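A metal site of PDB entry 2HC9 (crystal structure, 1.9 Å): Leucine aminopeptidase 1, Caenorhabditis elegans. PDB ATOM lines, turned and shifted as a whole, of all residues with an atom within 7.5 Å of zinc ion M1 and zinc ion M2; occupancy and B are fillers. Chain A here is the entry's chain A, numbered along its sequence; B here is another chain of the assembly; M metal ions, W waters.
Of the 25 residues printed, 4 come within 4 Å of zinc ion M1.
The backbone carbonyl oxygen of Asp 275 is in hydrogen-bond range of the backbone NH of Val 254.
N of Asp 257 lies within hydrogen-bond range of O of Met 272, 3.4 Å away.
NZ of Lys 264 is in salt-bridge range of OD2 of Asp 334, 2.9 Å away.
The side-chain amide nitrogen (ND2) of Asn 307 sits close to the side-chain carboxylate (OE2) of Glu 336, 3.4 Å away.
N of Asp 334 lies within hydrogen-bond range of O of Gly 259 (3.1 Å).
OD1 of Asp 257 lies within hydrogen-bond range of ND2 of Asn 307, at 2.9 Å.
The side-chain amino group (NZ) of Lys 266 of chain B is in salt-bridge range of the side-chain carboxylate (OD2) of Asp 334 (3.9 Å).
The side-chain carboxylate (OD1) of Asp 275 is in hydrogen-bond range of the side-chain hydroxyl (OG1) of Thr 362.
Zinc ion M1 is bound by OD2 of Asp 275 (2.0 Å), OE1 of Glu 336 (2.1 Å), water W1 (2.1 Å), NZ of Lys 252 (2.1 Å) and OD2 of Asp 257 (2.6 Å).
Within 4 Å of zinc ion M2: Asp 257, Asp 334 and Glu 336.
The nearest printed residue that does not touch zinc ion M2 is Lys 264 (4.2 Å).
Zinc ion M2 is bound by the side-chain carboxylate (OD1) of Asp 334 (2.0 Å), water W1 (2.0 Å), the side-chain carboxylate (OE2) of Glu 336 (2.0 Å), the side-chain carboxylate (OD2) of Asp 257 (2.1 Å) and the backbone carbonyl oxygen (O) of Asp 334 (2.2 Å).
Zinc ion M2 has five donor atoms within binding distance.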
ATOM      1  N   LYS A 252     -16.940  -1.761  18.630  1.00  0.00           N
ATOM      2  CA  LYS A 252     -18.113  -2.180  19.419  1.00  0.00           C
ATOM      3  C   LYS A 252     -18.872  -0.961  19.920  1.00  0.00           C
ATOM      4  O   LYS A 252     -18.335  -0.171  20.727  1.00  0.00           O
ATOM      5  CB  LYS A 252     -17.683  -3.011  20.646  1.00  0.00           C
ATOM      6  CG  LYS A 252     -18.864  -3.396  21.596  1.00  0.00           C
ATOM      7  CD  LYS A 252     -18.363  -4.188  22.806  1.00  0.00           C
ATOM      8  CE  LYS A 252     -19.550  -4.396  23.771  1.00  0.00           C
ATOM      9  NZ  LYS A 252     -19.169  -5.199  25.011  1.00  0.00           N
ATOM     10  N   VAL A 254     -21.970  -0.679  21.670  1.00  0.00           N
ATOM     11  CA  VAL A 254     -23.106  -1.002  22.526  1.00  0.00           C
ATOM     12  C   VAL A 254     -23.445   0.236  23.356  1.00  0.00           C
ATOM     13  O   VAL A 254     -22.771   0.555  24.337  1.00  0.00           O
ATOM     14  CB  VAL A 254     -22.829  -2.244  23.409  1.00  0.00           C
ATOM     15  CG1 VAL A 254     -24.018  -2.486  24.361  1.00  0.00           C
ATOM     16  CG2 VAL A 254     -22.617  -3.495  22.488  1.00  0.00           C
ATOM     17  N   TYR A 256     -25.814   0.956  25.339  1.00  0.00           N
ATOM     18  CA  TYR A 256     -25.998   0.582  26.742  1.00  0.00           C
ATOM     19  C   TYR A 256     -26.058  -0.908  26.831  1.00  0.00           C
ATOM     20  O   TYR A 256     -26.680  -1.547  25.997  1.00  0.00           O
ATOM     21  CB  TYR A 256     -27.310   1.150  27.308  1.00  0.00           C
ATOM     22  CG  TYR A 256     -27.291   1.125  28.803  1.00  0.00           C
ATOM     23  CD1 TYR A 256     -26.707   2.171  29.528  1.00  0.00           C
ATOM     24  CD2 TYR A 256     -27.816   0.039  29.515  1.00  0.00           C
ATOM     25  CE1 TYR A 256     -26.673   2.155  30.916  1.00  0.00           C
ATOM     26  CE2 TYR A 256     -27.804   0.012  30.889  1.00  0.00           C
ATOM     27  CZ  TYR A 256     -27.231   1.052  31.579  1.00  0.00           C
ATOM     28  OH  TYR A 256     -27.237   0.977  32.934  1.00  0.00           O
ATOM     29  N   ASP A 257     -25.422  -1.450  27.867  1.00  0.00           N
ATOM     30  CA  ASP A 257     -25.451  -2.894  28.088  1.00  0.00           C
ATOM     31  C   ASP A 257     -26.107  -3.200  29.456  1.00  0.00           C
ATOM     32  O   ASP A 257     -25.488  -3.066  30.501  1.00  0.00           O
ATOM     33  CB  ASP A 257     -24.016  -3.416  28.064  1.00  0.00           C
ATOM     34  CG  ASP A 257     -23.937  -4.923  27.968  1.00  0.00           C
ATOM     35  OD1 ASP A 257     -25.007  -5.589  27.861  1.00  0.00           O
ATOM     36  OD2 ASP A 257     -22.788  -5.419  27.995  1.00  0.00           O
ATOM     37  N   THR A 258     -27.375  -3.624  29.432  1.00  0.00           N
ATOM     38  CA  THR A 258     -28.018  -4.127  30.660  1.00  0.00           C
ATOM     39  C   THR A 258     -27.548  -5.547  31.004  1.00  0.00           C
ATOM     40  O   THR A 258     -27.861  -6.059  32.081  1.00  0.00           O
ATOM     41  CB  THR A 258     -29.541  -4.229  30.512  1.00  0.00           C
ATOM     42  OG1 THR A 258     -29.833  -5.222  29.527  1.00  0.00           O
ATOM     43  CG2 THR A 258     -30.179  -2.878  30.101  1.00  0.00           C
ATOM     44  N   GLY A 259     -26.821  -6.170  30.069  1.00  0.00           N
ATOM     45  CA  GLY A 259     -26.459  -7.587  30.159  1.00  0.00           C
ATOM     46  C   GLY A 259     -27.414  -8.486  29.359  1.00  0.00           C
ATOM     47  O   GLY A 259     -27.085  -9.628  28.999  1.00  0.00           O
ATOM     48  N   GLY A 260     -28.615  -7.959  29.098  1.00  0.00           N
ATOM     49  CA  GLY A 260     -29.677  -8.756  28.465  1.00  0.00           C
ATOM     50  C   GLY A 260     -30.409  -9.596  29.480  1.00  0.00           C
ATOM     51  O   GLY A 260     -30.379  -9.308  30.686  1.00  0.00           O
ATOM     52  N   GLN A 262     -29.707 -12.380  30.804  1.00  0.00           N
ATOM     53  CA  GLN A 262     -28.726 -12.667  31.864  1.00  0.00           C
ATOM     54  C   GLN A 262     -28.208 -11.328  32.387  1.00  0.00           C
ATOM     55  O   GLN A 262     -27.102 -10.885  32.072  1.00  0.00           O
ATOM     56  CB  GLN A 262     -27.603 -13.585  31.376  1.00  0.00           C
ATOM     57  CG  GLN A 262     -28.117 -15.038  31.190  1.00  0.00           C
ATOM     58  CD  GLN A 262     -27.239 -15.825  30.275  1.00  0.00           C
ATOM     59  OE1 GLN A 262     -27.187 -15.551  29.068  1.00  0.00           O
ATOM     60  NE2 GLN A 262     -26.534 -16.807  30.819  1.00  0.00           N
ATOM     61  N   LYS A 264     -27.152  -7.810  34.234  1.00  0.00           N
ATOM     62  CA  LYS A 264     -26.117  -7.343  35.150  1.00  0.00           C
ATOM     63  C   LYS A 264     -26.683  -7.055  36.536  1.00  0.00           C
ATOM     64  O   LYS A 264     -27.909  -6.908  36.715  1.00  0.00           O
ATOM     65  CB  LYS A 264     -25.439  -6.096  34.572  1.00  0.00           C
ATOM     66  CG  LYS A 264     -24.663  -6.440  33.285  1.00  0.00           C
ATOM     67  CD  LYS A 264     -23.954  -5.150  32.783  1.00  0.00           C
ATOM     68  CE  LYS A 264     -23.161  -5.435  31.494  1.00  0.00           C
ATOM     69  NZ  LYS A 264     -21.915  -6.283  31.810  1.00  0.00           N
ATOM     70  N   MET A 272     -22.568   1.341  32.301  1.00  0.00           N
ATOM     71  CA  MET A 272     -22.723   0.627  31.042  1.00  0.00           C
ATOM     72  C   MET A 272     -23.141   1.451  29.802  1.00  0.00           C
ATOM     73  O   MET A 272     -23.173   0.915  28.699  1.00  0.00           O
ATOM     74  CB  MET A 272     -23.608  -0.625  31.198  1.00  0.00           C
ATOM     75  CG  MET A 272     -22.950  -1.740  32.045  1.00  0.00           C
ATOM     76  SD  MET A 272     -21.374  -2.290  31.342  1.00  0.00           S
ATOM     77  CE  MET A 272     -20.190  -1.453  32.362  1.00  0.00           C
ATOM     78  N   ASP A 275     -20.188   1.247  27.193  1.00  0.00           N
ATOM     79  CA  ASP A 275     -19.932   0.035  26.419  1.00  0.00           C
ATOM     80  C   ASP A 275     -19.849   0.254  24.881  1.00  0.00           C
ATOM     81  O   ASP A 275     -19.753  -0.707  24.105  1.00  0.00           O
ATOM     82  CB  ASP A 275     -21.004  -1.011  26.759  1.00  0.00           C
ATOM     83  CG  ASP A 275     -20.511  -2.432  26.607  1.00  0.00           C
ATOM     84  OD1 ASP A 275     -19.302  -2.716  26.759  1.00  0.00           O
ATOM     85  OD2 ASP A 275     -21.377  -3.288  26.364  1.00  0.00           O
ATOM     86  N   MET A 276     -19.914   1.513  24.463  1.00  0.00           N
ATOM     87  CA  MET A 276     -19.703   1.906  23.059  1.00  0.00           C
ATOM     88  C   MET A 276     -18.350   2.618  22.873  1.00  0.00           C
ATOM     89  O   MET A 276     -18.100   3.235  21.813  1.00  0.00           O
ATOM     90  CB  MET A 276     -20.871   2.830  22.570  1.00  0.00           C
ATOM     91  CG  MET A 276     -21.387   3.889  23.585  1.00  0.00           C
ATOM     92  SD  MET A 276     -20.131   4.947  24.306  1.00  0.00           S
ATOM     93  CE  MET A 276     -19.734   5.898  22.807  1.00  0.00           C
ATOM     94  N   ASN A 307     -28.344  -3.387  24.235  1.00  0.00           N
ATOM     95  CA  ASN A 307     -28.581  -4.747  24.744  1.00  0.00           C
ATOM     96  C   ASN A 307     -29.536  -4.650  25.950  1.00  0.00           C
ATOM     97  O   ASN A 307     -29.111  -4.267  27.050  1.00  0.00           O
ATOM     98  CB  ASN A 307     -27.233  -5.397  25.129  1.00  0.00           C
ATOM     99  CG  ASN A 307     -27.341  -6.912  25.332  1.00  0.00           C
ATOM    100  OD1 ASN A 307     -28.198  -7.559  24.727  1.00  0.00           O
ATOM    101  ND2 ASN A 307     -26.503  -7.460  26.205  1.00  0.00           N
ATOM    102  N   ASN A 332     -24.570 -16.787  26.878  1.00  0.00           N
ATOM    103  CA  ASN A 332     -24.358 -15.608  27.692  1.00  0.00           C
ATOM    104  C   ASN A 332     -24.786 -14.356  26.916  1.00  0.00           C
ATOM    105  O   ASN A 332     -24.074 -13.865  26.042  1.00  0.00           O
ATOM    106  CB  ASN A 332     -22.889 -15.508  28.138  1.00  0.00           C
ATOM    107  CG  ASN A 332     -22.653 -14.369  29.110  1.00  0.00           C
ATOM    108  OD1 ASN A 332     -23.541 -13.559  29.388  1.00  0.00           O
ATOM    109  ND2 ASN A 332     -21.436 -14.297  29.623  1.00  0.00           N
ATOM    110  N   THR A 333     -25.950 -13.835  27.250  1.00  0.00           N
ATOM    111  CA  THR A 333     -26.498 -12.649  26.576  1.00  0.00           C
ATOM    112  C   THR A 333     -25.676 -11.412  26.846  1.00  0.00           C
ATOM    113  O   THR A 333     -25.808 -10.440  26.107  1.00  0.00           O
ATOM    114  CB  THR A 333     -27.964 -12.345  26.991  1.00  0.00           C
ATOM    115  OG1 THR A 333     -28.009 -12.040  28.394  1.00  0.00           O
ATOM    116  CG2 THR A 333     -28.870 -13.561  26.664  1.00  0.00           C
ATOM    117  N   ASP A 334     -24.845 -11.432  27.889  1.00  0.00           N
ATOM    118  CA  ASP A 334     -23.954 -10.299  28.234  1.00  0.00           C
ATOM    119  C   ASP A 334     -22.598 -10.406  27.486  1.00  0.00           C
ATOM    120  O   ASP A 334     -21.749  -9.514  27.565  1.00  0.00           O
ATOM    121  CB  ASP A 334     -23.722 -10.306  29.747  1.00  0.00           C
ATOM    122  CG  ASP A 334     -23.203  -8.978  30.292  1.00  0.00           C
ATOM    123  OD1 ASP A 334     -23.059  -7.978  29.536  1.00  0.00           O
ATOM    124  OD2 ASP A 334     -22.940  -8.924  31.498  1.00  0.00           O
ATOM    125  N   ALA A 335     -22.388 -11.509  26.772  1.00  0.00           N
ATOM    126  CA  ALA A 335     -21.210 -11.647  25.913  1.00  0.00           C
ATOM    127  C   ALA A 335     -21.650 -11.243  24.491  1.00  0.00           C
ATOM    128  O   ALA A 335     -21.513 -12.007  23.502  1.00  0.00           O
ATOM    129  CB  ALA A 335     -20.698 -13.116  25.961  1.00  0.00           C
ATOM    130  N   GLU A 336     -22.206 -10.027  24.411  1.00  0.00           N
ATOM    131  CA  GLU A 336     -22.900  -9.563  23.194  1.00  0.00           C
ATOM    132  C   GLU A 336     -21.973  -8.807  22.237  1.00  0.00           C
ATOM    133  O   GLU A 336     -22.188  -8.820  20.994  1.00  0.00           O
ATOM    134  CB  GLU A 336     -24.155  -8.726  23.551  1.00  0.00           C
ATOM    135  CG  GLU A 336     -23.886  -7.204  23.729  1.00  0.00           C
ATOM    136  CD  GLU A 336     -23.045  -6.901  24.949  1.00  0.00           C
ATOM    137  OE1 GLU A 336     -22.296  -5.899  24.953  1.00  0.00           O
ATOM    138  OE2 GLU A 336     -23.118  -7.667  25.929  1.00  0.00           O
ATOM    139  N   GLY A 337     -20.956  -8.137  22.784  1.00  0.00           N
ATOM    140  CA  GLY A 337     -19.996  -7.406  21.941  1.00  0.00           C
ATOM    141  C   GLY A 337     -19.315  -8.316  20.919  1.00  0.00           C
ATOM    142  O   GLY A 337     -19.156  -7.951  19.757  1.00  0.00           O
ATOM    143  N   ARG A 338     -18.950  -9.502  21.346  1.00  0.00           N
ATOM    144  CA  ARG A 338     -18.228 -10.406  20.472  1.00  0.00           C
ATOM    145  C   ARG A 338     -19.128 -10.915  19.323  1.00  0.00           C
ATOM    146  O   ARG A 338     -18.639 -11.158  18.219  1.00  0.00           O
ATOM    147  CB  ARG A 338     -17.612 -11.568  21.264  1.00  0.00           C
ATOM    148  CG  ARG A 338     -18.675 -12.502  21.925  1.00  0.00           C
ATOM    149  CD  ARG A 338     -18.007 -13.406  22.997  1.00  0.00           C
ATOM    150  NE  ARG A 338     -17.726 -12.626  24.216  1.00  0.00           N
ATOM    151  CZ  ARG A 338     -17.280 -13.172  25.346  1.00  0.00           C
ATOM    152  NH1 ARG A 338     -17.096 -14.501  25.420  1.00  0.00           N
ATOM    153  NH2 ARG A 338     -17.069 -12.406  26.411  1.00  0.00           N
ATOM    154  N   ILE A 340     -21.637  -9.082  17.901  1.00  0.00           N
ATOM    155  CA  ILE A 340     -21.786  -8.020  16.911  1.00  0.00           C
ATOM    156  C   ILE A 340     -20.494  -7.806  16.122  1.00  0.00           C
ATOM    157  O   ILE A 340     -20.542  -7.522  14.908  1.00  0.00           O
ATOM    158  CB  ILE A 340     -22.385  -6.715  17.507  1.00  0.00           C
ATOM    159  CG1 ILE A 340     -21.344  -5.966  18.361  1.00  0.00           C
ATOM    160  CG2 ILE A 340     -23.666  -7.037  18.335  1.00  0.00           C
ATOM    161  CD1 ILE A 340     -21.852  -4.587  18.925  1.00  0.00           C
ATOM    162  N   THR A 362     -14.786  -2.357  24.301  1.00  0.00           N
ATOM    163  CA  THR A 362     -14.825  -2.501  25.765  1.00  0.00           C
ATOM    164  C   THR A 362     -15.458  -3.866  26.043  1.00  0.00           C
ATOM    165  O   THR A 362     -16.664  -3.969  26.289  1.00  0.00           O
ATOM    166  CB  THR A 362     -15.688  -1.378  26.412  1.00  0.00           C
ATOM    167  OG1 THR A 362     -16.963  -1.354  25.783  1.00  0.00           O
ATOM    168  CG2 THR A 362     -15.034  -0.032  26.205  1.00  0.00           C
ATOM    169  N   LEU A 363     -14.664  -4.938  25.940  1.00  0.00           N
ATOM    170  CA  LEU A 363     -15.257  -6.244  25.720  1.00  0.00           C
ATOM    171  C   LEU A 363     -15.531  -6.997  27.033  1.00  0.00           C
ATOM    172  O   LEU A 363     -16.617  -7.538  27.218  1.00  0.00           O
ATOM    173  CB  LEU A 363     -14.424  -7.112  24.737  1.00  0.00           C
ATOM    174  CG  LEU A 363     -15.254  -8.246  24.116  1.00  0.00           C
ATOM    175  CD1 LEU A 363     -16.403  -7.718  23.225  1.00  0.00           C
ATOM    176  CD2 LEU A 363     -14.333  -9.156  23.304  1.00  0.00           C
ATOM    177  N   THR A 364     -14.541  -7.044  27.927  1.00  0.00           N
ATOM    178  CA  THR A 364     -14.610  -7.941  29.110  1.00  0.00           C
ATOM    179  C   THR A 364     -14.098  -7.255  30.367  1.00  0.00           C
ATOM    180  O   THR A 364     -13.117  -6.535  30.324  1.00  0.00           O
ATOM    181  CB  THR A 364     -13.797  -9.258  28.895  1.00  0.00           C
ATOM    182  OG1 THR A 364     -12.384  -8.970  28.733  1.00  0.00           O
ATOM    183  CG2 THR A 364     -14.309 -10.000  27.655  1.00  0.00           C
ATOM    184  N   LYS B 266     -27.581 -15.720  36.133  1.00  0.00           N
ATOM    185  CA  LYS B 266     -26.743 -15.865  34.937  1.00  0.00           C
ATOM    186  C   LYS B 266     -26.415 -17.326  34.632  1.00  0.00           C
ATOM    187  O   LYS B 266     -26.414 -17.745  33.467  1.00  0.00           O
ATOM    188  CB  LYS B 266     -25.440 -15.086  35.116  1.00  0.00           C
ATOM    189  CG  LYS B 266     -24.528 -15.159  33.889  1.00  0.00           C
ATOM    190  CD  LYS B 266     -23.442 -14.091  33.966  1.00  0.00           C
ATOM    191  CE  LYS B 266     -23.244 -13.400  32.621  1.00  0.00           C
ATOM    192  NZ  LYS B 266     -22.005 -12.524  32.620  1.00  0.00           N
HETATM  193 ZN    ZN M   1     -20.880  -5.191  26.260  1.00  0.00          ZN
HETATM  194 ZN    ZN M   2     -22.312  -7.407  27.788  1.00  0.00          ZN
HETATM  195  O   HOH W   1     -20.398  -6.810  27.483  1.00  0.00           O
